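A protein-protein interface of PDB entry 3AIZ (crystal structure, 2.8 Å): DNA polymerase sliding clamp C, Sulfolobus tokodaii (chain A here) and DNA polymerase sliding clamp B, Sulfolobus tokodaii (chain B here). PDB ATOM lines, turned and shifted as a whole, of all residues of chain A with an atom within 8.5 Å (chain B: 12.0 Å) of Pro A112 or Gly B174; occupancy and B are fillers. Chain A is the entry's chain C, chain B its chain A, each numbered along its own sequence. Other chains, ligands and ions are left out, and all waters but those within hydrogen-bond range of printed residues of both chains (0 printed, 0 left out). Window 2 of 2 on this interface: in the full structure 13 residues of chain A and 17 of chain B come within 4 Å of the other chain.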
ATOM      1  N   GLU A  24     -20.978   1.154   0.789  1.00  0.00           N
ATOM      2  CA  GLU A  24     -21.773   1.245  -0.429  1.00  0.00           C
ATOM      3  C   GLU A  24     -23.212   1.606  -0.094  1.00  0.00           C
ATOM      4  O   GLU A  24     -23.798   1.054   0.835  1.00  0.00           O
ATOM      5  CB  GLU A  24     -21.724  -0.078  -1.200  1.00  0.00           C
ATOM      6  CG  GLU A  24     -22.708  -0.175  -2.364  1.00  0.00           C
ATOM      7  CD  GLU A  24     -24.087  -0.665  -1.943  1.00  0.00           C
ATOM      8  OE1 GLU A  24     -24.167  -1.545  -1.057  1.00  0.00           O
ATOM      9  OE2 GLU A  24     -25.092  -0.176  -2.505  1.00  0.00           O
ATOM     10  N   VAL A  67     -29.780   2.266  -8.085  1.00  0.00           N
ATOM     11  CA  VAL A  67     -28.399   2.355  -8.536  1.00  0.00           C
ATOM     12  C   VAL A  67     -27.449   2.471  -7.351  1.00  0.00           C
ATOM     13  O   VAL A  67     -27.416   3.491  -6.664  1.00  0.00           O
ATOM     14  CB  VAL A  67     -28.188   3.538  -9.506  1.00  0.00           C
ATOM     15  CG1 VAL A  67     -28.895   4.783  -8.996  1.00  0.00           C
ATOM     16  CG2 VAL A  67     -26.703   3.797  -9.712  1.00  0.00           C
ATOM     17  N   GLY A  68     -26.684   1.414  -7.108  1.00  0.00           N
ATOM     18  CA  GLY A  68     -25.711   1.416  -6.033  1.00  0.00           C
ATOM     19  C   GLY A  68     -24.413   2.062  -6.473  1.00  0.00           C
ATOM     20  O   GLY A  68     -24.084   2.064  -7.657  1.00  0.00           O
ATOM     21  N   VAL A  69     -23.672   2.609  -5.517  1.00  0.00           N
ATOM     22  CA  VAL A  69     -22.406   3.263  -5.821  1.00  0.00           C
ATOM     23  C   VAL A  69     -21.518   3.355  -4.585  1.00  0.00           C
ATOM     24  O   VAL A  69     -22.002   3.608  -3.483  1.00  0.00           O
ATOM     25  CB  VAL A  69     -22.631   4.678  -6.394  1.00  0.00           C
ATOM     26  CG1 VAL A  69     -23.390   5.544  -5.396  1.00  0.00           C
ATOM     27  CG2 VAL A  69     -21.305   5.320  -6.768  1.00  0.00           C
ATOM     28  N   LYS A  70     -20.220   3.135  -4.771  1.00  0.00           N
ATOM     29  CA  LYS A  70     -19.262   3.280  -3.682  1.00  0.00           C
ATOM     30  C   LYS A  70     -19.360   4.690  -3.106  1.00  0.00           C
ATOM     31  O   LYS A  70     -19.119   5.673  -3.804  1.00  0.00           O
ATOM     32  CB  LYS A  70     -17.841   3.004  -4.174  1.00  0.00           C
ATOM     33  CG  LYS A  70     -16.781   3.092  -3.087  1.00  0.00           C
ATOM     34  CD  LYS A  70     -15.381   2.937  -3.660  1.00  0.00           C
ATOM     35  CE  LYS A  70     -14.323   3.078  -2.576  1.00  0.00           C
ATOM     36  NZ  LYS A  70     -12.942   3.063  -3.135  1.00  0.00           N
ATOM     37  N   ASP A  73     -16.231   7.483  -3.322  1.00  0.00           N
ATOM     38  CA  ASP A  73     -16.032   8.181  -4.584  1.00  0.00           C
ATOM     39  C   ASP A  73     -17.130   9.209  -4.812  1.00  0.00           C
ATOM     40  O   ASP A  73     -16.869  10.319  -5.278  1.00  0.00           O
ATOM     41  CB  ASP A  73     -16.002   7.185  -5.743  1.00  0.00           C
ATOM     42  CG  ASP A  73     -14.833   6.230  -5.655  1.00  0.00           C
ATOM     43  OD1 ASP A  73     -13.812   6.598  -5.033  1.00  0.00           O
ATOM     44  OD2 ASP A  73     -14.933   5.115  -6.208  1.00  0.00           O
ATOM     45  N   ASP A  92     -26.820   7.149 -17.319  1.00  0.00           N
ATOM     46  CA  ASP A  92     -26.390   7.149 -18.715  1.00  0.00           C
ATOM     47  C   ASP A  92     -26.785   5.874 -19.459  1.00  0.00           C
ATOM     48  O   ASP A  92     -26.071   5.427 -20.357  1.00  0.00           O
ATOM     49  CB  ASP A  92     -24.875   7.365 -18.811  1.00  0.00           C
ATOM     50  CG  ASP A  92     -24.082   6.274 -18.115  1.00  0.00           C
ATOM     51  OD1 ASP A  92     -24.680   5.247 -17.730  1.00  0.00           O
ATOM     52  OD2 ASP A  92     -22.854   6.444 -17.954  1.00  0.00           O
ATOM     53  N   ASN A  94     -26.275   3.026 -19.295  1.00  0.00           N
ATOM     54  CA  ASN A  94     -25.382   1.967 -18.839  1.00  0.00           C
ATOM     55  C   ASN A  94     -25.504   1.764 -17.334  1.00  0.00           C
ATOM     56  O   ASN A  94     -24.634   1.159 -16.704  1.00  0.00           O
ATOM     57  CB  ASN A  94     -23.931   2.276 -19.216  1.00  0.00           C
ATOM     58  CG  ASN A  94     -23.639   2.007 -20.679  1.00  0.00           C
ATOM     59  OD1 ASN A  94     -24.471   1.455 -21.400  1.00  0.00           O
ATOM     60  ND2 ASN A  94     -22.447   2.390 -21.126  1.00  0.00           N
ATOM     61  N   GLN A  95     -26.589   2.287 -16.769  1.00  0.00           N
ATOM     62  CA  GLN A  95     -26.875   2.162 -15.344  1.00  0.00           C
ATOM     63  C   GLN A  95     -25.926   2.999 -14.487  1.00  0.00           C
ATOM     64  O   GLN A  95     -26.185   3.232 -13.307  1.00  0.00           O
ATOM     65  CB  GLN A  95     -26.847   0.692 -14.912  1.00  0.00           C
ATOM     66  CG  GLN A  95     -27.926  -0.163 -15.565  1.00  0.00           C
ATOM     67  CD  GLN A  95     -27.801  -1.634 -15.215  1.00  0.00           C
ATOM     68  OE1 GLN A  95     -26.720  -2.114 -14.870  1.00  0.00           O
ATOM     69  NE2 GLN A  95     -28.911  -2.360 -15.305  1.00  0.00           N
ATOM     70  N   ASN A  96     -24.833   3.456 -15.090  1.00  0.00           N
ATOM     71  CA  ASN A  96     -23.859   4.284 -14.388  1.00  0.00           C
ATOM     72  C   ASN A  96     -24.453   5.613 -13.933  1.00  0.00           C
ATOM     73  O   ASN A  96     -25.163   6.279 -14.684  1.00  0.00           O
ATOM     74  CB  ASN A  96     -22.633   4.529 -15.269  1.00  0.00           C
ATOM     75  CG  ASN A  96     -21.873   3.254 -15.575  1.00  0.00           C
ATOM     76  OD1 ASN A  96     -21.093   3.195 -16.528  1.00  0.00           O
ATOM     77  ND2 ASN A  96     -22.099   2.222 -14.768  1.00  0.00           N
ATOM     78  N   ILE A  97     -24.155   5.993 -12.695  1.00  0.00           N
ATOM     79  CA  ILE A  97     -24.664   7.236 -12.130  1.00  0.00           C
ATOM     80  C   ILE A  97     -23.861   8.440 -12.627  1.00  0.00           C
ATOM     81  O   ILE A  97     -22.635   8.379 -12.739  1.00  0.00           O
ATOM     82  CB  ILE A  97     -24.650   7.192 -10.585  1.00  0.00           C
ATOM     83  CG1 ILE A  97     -25.358   8.414  -9.998  1.00  0.00           C
ATOM     84  CG2 ILE A  97     -23.226   7.080 -10.060  1.00  0.00           C
ATOM     85  CD1 ILE A  97     -26.851   8.429 -10.241  1.00  0.00           C
ATOM     86  N   LYS A  98     -24.559   9.528 -12.936  1.00  0.00           N
ATOM     87  CA  LYS A  98     -23.918  10.755 -13.399  1.00  0.00           C
ATOM     88  C   LYS A  98     -24.138  11.906 -12.425  1.00  0.00           C
ATOM     89  O   LYS A  98     -25.274  12.253 -12.106  1.00  0.00           O
ATOM     90  CB  LYS A  98     -24.441  11.156 -14.780  1.00  0.00           C
ATOM     91  CG  LYS A  98     -23.733  10.489 -15.944  1.00  0.00           C
ATOM     92  CD  LYS A  98     -24.180  11.091 -17.269  1.00  0.00           C
ATOM     93  CE  LYS A  98     -23.409  10.498 -18.438  1.00  0.00           C
ATOM     94  NZ  LYS A  98     -23.904  11.006 -19.749  1.00  0.00           N
ATOM     95  N   PHE A 109     -18.986  14.042 -13.264  1.00  0.00           N
ATOM     96  CA  PHE A 109     -18.315  12.824 -12.831  1.00  0.00           C
ATOM     97  C   PHE A 109     -19.222  11.622 -13.074  1.00  0.00           C
ATOM     98  O   PHE A 109     -20.446  11.733 -13.008  1.00  0.00           O
ATOM     99  CB  PHE A 109     -17.959  12.903 -11.346  1.00  0.00           C
ATOM    100  CG  PHE A 109     -16.948  13.961 -11.014  1.00  0.00           C
ATOM    101  CD1 PHE A 109     -17.336  15.277 -10.831  1.00  0.00           C
ATOM    102  CD2 PHE A 109     -15.610  13.637 -10.864  1.00  0.00           C
ATOM    103  CE1 PHE A 109     -16.410  16.250 -10.519  1.00  0.00           C
ATOM    104  CE2 PHE A 109     -14.679  14.606 -10.551  1.00  0.00           C
ATOM    105  CZ  PHE A 109     -15.078  15.914 -10.379  1.00  0.00           C
ATOM    106  N   THR A 110     -18.621  10.473 -13.355  1.00  0.00           N
ATOM    107  CA  THR A 110     -19.383   9.250 -13.569  1.00  0.00           C
ATOM    108  C   THR A 110     -18.811   8.099 -12.753  1.00  0.00           C
ATOM    109  O   THR A 110     -17.598   7.915 -12.686  1.00  0.00           O
ATOM    110  CB  THR A 110     -19.423   8.857 -15.056  1.00  0.00           C
ATOM    111  OG1 THR A 110     -20.345   9.708 -15.748  1.00  0.00           O
ATOM    112  CG2 THR A 110     -19.869   7.413 -15.213  1.00  0.00           C
ATOM    113  N   PHE A 111     -19.694   7.330 -12.127  1.00  0.00           N
ATOM    114  CA  PHE A 111     -19.274   6.200 -11.312  1.00  0.00           C
ATOM    115  C   PHE A 111     -19.851   4.904 -11.860  1.00  0.00           C
ATOM    116  O   PHE A 111     -21.000   4.867 -12.298  1.00  0.00           O
ATOM    117  CB  PHE A 111     -19.711   6.403  -9.860  1.00  0.00           C
ATOM    118  CG  PHE A 111     -19.290   7.723  -9.283  1.00  0.00           C
ATOM    119  CD1 PHE A 111     -20.152   8.807  -9.301  1.00  0.00           C
ATOM    120  CD2 PHE A 111     -18.030   7.883  -8.731  1.00  0.00           C
ATOM    121  CE1 PHE A 111     -19.766  10.027  -8.774  1.00  0.00           C
ATOM    122  CE2 PHE A 111     -17.638   9.100  -8.202  1.00  0.00           C
ATOM    123  CZ  PHE A 111     -18.508  10.173  -8.223  1.00  0.00           C
ATOM    124  N   PRO A 112     -19.048   3.832 -11.844  1.00  0.00           N
ATOM    125  CA  PRO A 112     -19.517   2.525 -12.307  1.00  0.00           C
ATOM    126  C   PRO A 112     -20.546   1.960 -11.339  1.00  0.00           C
ATOM    127  O   PRO A 112     -20.446   2.198 -10.134  1.00  0.00           O
ATOM    128  CB  PRO A 112     -18.246   1.674 -12.273  1.00  0.00           C
ATOM    129  CG  PRO A 112     -17.413   2.304 -11.211  1.00  0.00           C
ATOM    130  CD  PRO A 112     -17.661   3.778 -11.350  1.00  0.00           C
ATOM    131  N   SER A 113     -21.527   1.231 -11.858  1.00  0.00           N
ATOM    132  CA  SER A 113     -22.523   0.598 -11.005  1.00  0.00           C
ATOM    133  C   SER A 113     -21.948  -0.651 -10.350  1.00  0.00           C
ATOM    134  O   SER A 113     -21.100  -1.335 -10.927  1.00  0.00           O
ATOM    135  CB  SER A 113     -23.778   0.248 -11.804  1.00  0.00           C
ATOM    136  OG  SER A 113     -24.423   1.420 -12.268  1.00  0.00           O
ATOM    137  N   ILE A 114     -22.410  -0.936  -9.138  1.00  0.00           N
ATOM    138  CA  ILE A 114     -21.950  -2.103  -8.396  1.00  0.00           C
ATOM    139  C   ILE A 114     -23.136  -2.869  -7.823  1.00  0.00           C
ATOM    140  O   ILE A 114     -24.252  -2.352  -7.773  1.00  0.00           O
ATOM    141  CB  ILE A 114     -21.002  -1.698  -7.254  1.00  0.00           C
ATOM    142  CG1 ILE A 114     -21.671  -0.657  -6.356  1.00  0.00           C
ATOM    143  CG2 ILE A 114     -19.699  -1.149  -7.813  1.00  0.00           C
ATOM    144  CD1 ILE A 114     -20.758  -0.105  -5.285  1.00  0.00           C
ATOM    145  N   VAL A 115     -22.895  -4.105  -7.398  1.00  0.00           N
ATOM    146  CA  VAL A 115     -23.950  -4.919  -6.809  1.00  0.00           C
ATOM    147  C   VAL A 115     -24.474  -4.280  -5.526  1.00  0.00           C
ATOM    148  O   VAL A 115     -23.710  -3.982  -4.608  1.00  0.00           O
ATOM    149  CB  VAL A 115     -23.479  -6.357  -6.522  1.00  0.00           C
ATOM    150  CG1 VAL A 115     -23.307  -7.124  -7.822  1.00  0.00           C
ATOM    151  CG2 VAL A 115     -22.184  -6.348  -5.727  1.00  0.00           C
ATOM    152  N   LEU B 152      -8.819  13.305  -8.773  1.00  0.00           N
ATOM    153  CA  LEU B 152      -9.777  12.317  -8.297  1.00  0.00           C
ATOM    154  C   LEU B 152      -9.886  11.121  -9.234  1.00  0.00           C
ATOM    155  O   LEU B 152      -9.920   9.977  -8.785  1.00  0.00           O
ATOM    156  CB  LEU B 152     -11.158  12.946  -8.104  1.00  0.00           C
ATOM    157  CG  LEU B 152     -11.349  13.846  -6.882  1.00  0.00           C
ATOM    158  CD1 LEU B 152     -12.747  14.443  -6.875  1.00  0.00           C
ATOM    159  CD2 LEU B 152     -11.089  13.067  -5.606  1.00  0.00           C
ATOM    160  N   VAL B 153      -9.932  11.385 -10.535  1.00  0.00           N
ATOM    161  CA  VAL B 153     -10.254  10.336 -11.498  1.00  0.00           C
ATOM    162  C   VAL B 153      -9.073   9.841 -12.339  1.00  0.00           C
ATOM    163  O   VAL B 153      -8.308   8.982 -11.905  1.00  0.00           O
ATOM    164  CB  VAL B 153     -11.393  10.775 -12.439  1.00  0.00           C
ATOM    165  CG1 VAL B 153     -12.004   9.564 -13.123  1.00  0.00           C
ATOM    166  CG2 VAL B 153     -12.452  11.537 -11.666  1.00  0.00           C
ATOM    167  N   GLY B 154      -8.936  10.392 -13.541  1.00  0.00           N
ATOM    168  CA  GLY B 154      -8.080   9.811 -14.563  1.00  0.00           C
ATOM    169  C   GLY B 154      -6.585   9.795 -14.316  1.00  0.00           C
ATOM    170  O   GLY B 154      -6.113  10.035 -13.204  1.00  0.00           O
ATOM    171  N   GLU B 155      -5.838   9.500 -15.377  1.00  0.00           N
ATOM    172  CA  GLU B 155      -4.381   9.499 -15.337  1.00  0.00           C
ATOM    173  C   GLU B 155      -3.836  10.328 -16.499  1.00  0.00           C
ATOM    174  O   GLU B 155      -2.696  10.791 -16.470  1.00  0.00           O
ATOM    175  CB  GLU B 155      -3.845   8.068 -15.394  1.00  0.00           C
ATOM    176  CG  GLU B 155      -2.355   7.945 -15.106  1.00  0.00           C
ATOM    177  CD  GLU B 155      -1.927   6.510 -14.851  1.00  0.00           C
ATOM    178  OE1 GLU B 155      -2.811   5.633 -14.739  1.00  0.00           O
ATOM    179  OE2 GLU B 155      -0.706   6.259 -14.756  1.00  0.00           O
ATOM    180  N   SER B 169     -11.240  15.849 -20.354  1.00  0.00           N
ATOM    181  CA  SER B 169     -11.787  14.523 -20.072  1.00  0.00           C
ATOM    182  C   SER B 169     -10.747  13.546 -19.536  1.00  0.00           C
ATOM    183  O   SER B 169      -9.607  13.522 -19.996  1.00  0.00           O
ATOM    184  CB  SER B 169     -12.428  13.935 -21.330  1.00  0.00           C
ATOM    185  OG  SER B 169     -13.522  14.723 -21.764  1.00  0.00           O
ATOM    186  N   THR B 170     -11.154  12.735 -18.565  1.00  0.00           N
ATOM    187  CA  THR B 170     -10.306  11.671 -18.039  1.00  0.00           C
ATOM    188  C   THR B 170     -11.133  10.429 -17.729  1.00  0.00           C
ATOM    189  O   THR B 170     -12.350  10.511 -17.561  1.00  0.00           O
ATOM    190  CB  THR B 170      -9.563  12.105 -16.763  1.00  0.00           C
ATOM    191  OG1 THR B 170     -10.512  12.458 -15.748  1.00  0.00           O
ATOM    192  CG2 THR B 170      -8.669  13.294 -17.048  1.00  0.00           C
ATOM    193  N   GLU B 171     -10.465   9.283 -17.652  1.00  0.00           N
ATOM    194  CA  GLU B 171     -11.137   8.018 -17.384  1.00  0.00           C
ATOM    195  C   GLU B 171     -10.215   7.069 -16.629  1.00  0.00           C
ATOM    196  O   GLU B 171      -9.074   6.851 -17.032  1.00  0.00           O
ATOM    197  CB  GLU B 171     -11.602   7.374 -18.694  1.00  0.00           C
ATOM    198  CG  GLU B 171     -12.391   6.077 -18.522  1.00  0.00           C
ATOM    199  CD  GLU B 171     -11.508   4.877 -18.212  1.00  0.00           C
ATOM    200  OE1 GLU B 171     -10.371   4.823 -18.730  1.00  0.00           O
ATOM    201  OE2 GLU B 171     -11.956   3.984 -17.457  1.00  0.00           O
ATOM    202  N   GLU B 172     -10.712   6.503 -15.534  1.00  0.00           N
ATOM    203  CA  GLU B 172      -9.935   5.542 -14.762  1.00  0.00           C
ATOM    204  C   GLU B 172     -10.818   4.599 -13.954  1.00  0.00           C
ATOM    205  O   GLU B 172     -11.693   5.038 -13.210  1.00  0.00           O
ATOM    206  CB  GLU B 172      -8.958   6.257 -13.828  1.00  0.00           C
ATOM    207  CG  GLU B 172      -8.057   5.310 -13.051  1.00  0.00           C
ATOM    208  CD  GLU B 172      -7.207   6.019 -12.017  1.00  0.00           C
ATOM    209  OE1 GLU B 172      -5.972   6.078 -12.199  1.00  0.00           O
ATOM    210  OE2 GLU B 172      -7.773   6.519 -11.022  1.00  0.00           O
ATOM    211  N   ALA B 173     -10.575   3.300 -14.108  1.00  0.00           N
ATOM    212  CA  ALA B 173     -11.262   2.278 -13.323  1.00  0.00           C
ATOM    213  C   ALA B 173     -12.781   2.430 -13.350  1.00  0.00           C
ATOM    214  O   ALA B 173     -13.444   2.290 -12.321  1.00  0.00           O
ATOM    215  CB  ALA B 173     -10.752   2.282 -11.886  1.00  0.00           C
ATOM    216  N   GLY B 174     -13.325   2.716 -14.528  1.00  0.00           N
ATOM    217  CA  GLY B 174     -14.762   2.832 -14.692  1.00  0.00           C
ATOM    218  C   GLY B 174     -15.299   4.204 -14.339  1.00  0.00           C
ATOM    219  O   GLY B 174     -16.444   4.530 -14.653  1.00  0.00           O
ATOM    220  N   ARG B 175     -14.475   5.010 -13.679  1.00  0.00           N
ATOM    221  CA  ARG B 175     -14.863   6.371 -13.331  1.00  0.00           C
ATOM    222  C   ARG B 175     -14.513   7.351 -14.447  1.00  0.00           C
ATOM    223  O   ARG B 175     -13.523   7.176 -15.156  1.00  0.00           O
ATOM    224  CB  ARG B 175     -14.239   6.795 -11.999  1.00  0.00           C
ATOM    225  CG  ARG B 175     -14.896   6.136 -10.795  1.00  0.00           C
ATOM    226  CD  ARG B 175     -14.293   6.596  -9.481  1.00  0.00           C
ATOM    227  NE  ARG B 175     -12.911   6.159  -9.326  1.00  0.00           N
ATOM    228  CZ  ARG B 175     -11.869   6.983  -9.296  1.00  0.00           C
ATOM    229  NH1 ARG B 175     -12.055   8.292  -9.402  1.00  0.00           N
ATOM    230  NH2 ARG B 175     -10.642   6.499  -9.154  1.00  0.00           N
ATOM    231  N   THR B 176     -15.342   8.377 -14.601  1.00  0.00           N
ATOM    232  CA  THR B 176     -15.198   9.324 -15.698  1.00  0.00           C
ATOM    233  C   THR B 176     -15.317  10.766 -15.224  1.00  0.00           C
ATOM    234  O   THR B 176     -16.089  11.067 -14.316  1.00  0.00           O
ATOM    235  CB  THR B 176     -16.253   9.063 -16.793  1.00  0.00           C
ATOM    236  OG1 THR B 176     -15.646   8.365 -17.886  1.00  0.00           O
ATOM    237  CG2 THR B 176     -16.843  10.373 -17.300  1.00  0.00           C
ATOM    238  N   TYR B 177     -14.543  11.652 -15.842  1.00  0.00           N
ATOM    239  CA  TYR B 177     -14.628  13.080 -15.560  1.00  0.00           C
ATOM    240  C   TYR B 177     -14.641  13.880 -16.856  1.00  0.00           C
ATOM    241  O   TYR B 177     -13.907  13.570 -17.793  1.00  0.00           O
ATOM    242  CB  TYR B 177     -13.462  13.532 -14.681  1.00  0.00           C
ATOM    243  CG  TYR B 177     -13.363  15.034 -14.529  1.00  0.00           C
ATOM    244  CD1 TYR B 177     -14.175  15.716 -13.633  1.00  0.00           C
ATOM    245  CD2 TYR B 177     -12.458  15.771 -15.279  1.00  0.00           C
ATOM    246  CE1 TYR B 177     -14.089  17.087 -13.489  1.00  0.00           C
ATOM    247  CE2 TYR B 177     -12.364  17.142 -15.142  1.00  0.00           C
ATOM    248  CZ  TYR B 177     -13.181  17.795 -14.245  1.00  0.00           C
ATOM    249  OH  TYR B 177     -13.091  19.162 -14.104  1.00  0.00           O
ATOM    250  N   LYS B 178     -15.479  14.909 -16.902  1.00  0.00           N
ATOM    251  CA  LYS B 178     -15.569  15.766 -18.077  1.00  0.00           C
ATOM    252  C   LYS B 178     -16.106  17.149 -17.723  1.00  0.00           C
ATOM    253  O   LYS B 178     -17.292  17.309 -17.437  1.00  0.00           O
ATOM    254  CB  LYS B 178     -16.449  15.119 -19.148  1.00  0.00           C
ATOM    255  CG  LYS B 178     -16.555  15.929 -20.431  1.00  0.00           C
ATOM    256  CD  LYS B 178     -17.472  15.254 -21.439  1.00  0.00           C
ATOM    257  CE  LYS B 178     -16.978  13.857 -21.789  1.00  0.00           C
ATOM    258  NZ  LYS B 178     -17.906  13.157 -22.722  1.00  0.00           N
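N of Thr A110 is in hydrogen-bond range of O of Thr B176. The guanidinium group (NE) of Arg B175 lies within salt-bridge range of the side-chain carboxylate (OD2) of Asp A73 (3.9 Å).
The guanidinium group (NH2) of Arg B175 lies within salt-bridge range of the side-chain carboxylate (OE2) of Glu B172, 3.4 Å away. NH1 of Arg B175 sits at hydrogen-bond distance from O of Leu B152, at 2.8 Å. N of Gly B174 sits at hydrogen-bond distance from OE2 of Glu B171 (3.5 Å). The backbone carbonyl oxygen (O) of Tyr B177 sits at hydrogen-bond distance from the backbone NH (N) of Thr B170 (3.0 Å). The side-chain carboxylate of Glu B172 lies close to the backbone carbonyl oxygen of Val B153 (2.7 Å).
Among the printed residues, pairs that only touch across the chains: Phe A109 with Val B153, Phe A109 with Thr B176, Phe A109 with Tyr B177, Thr A110 with Arg B175, Pro A112 with Gly B174 and Pro A112 with Arg B175.
No residue of chain B comes within 4 Å of Val A69. No residue of chain B comes within 4 Å of Asn A96. Of the printed residues of chain B, Phe A109 touches Val B153 (3.9 Å), Thr B176 (3.2 Å) and Tyr B177 (3.3 Å). Thr A110 touches just these residues of chain B: Arg B175 and Thr B176. Phe A111 touches none of the printed residues of chain B. Pro A112 touches just these residues of chain B: Gly B174 and Arg B175. No residue of chain B comes within 4 Å of Ser A113. Of the printed residues of chain A, Val B153 touches Phe A109. No residue of chain A comes within 4 Å of Ala B173. Of chain A, only Pro A112 comes within 4 Å of Gly B174. Of the printed residues of chain A, Arg B175 touches Asp A73 (3.6 Å), Thr A110 (3.2 Å) and Pro A112 (3.7 Å). Printed residues of chain A within 4 Å of Tyr B177: Phe A109 (3.3 Å). The nearest residue of chain A that does not touch Gly B174 is Thr A110 (4.1 Å). The nearest printed residue of chain A that does not touch Val B153 is Thr A110 (5.8 Å).
Hydrophobic or aromatic side chains of chain A that line the printed part of chain B: Phe A109 and Pro A112. Hydrophobic or aromatic side chains of chain B that line the printed part of chain A: Val B153 and Tyr B177.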
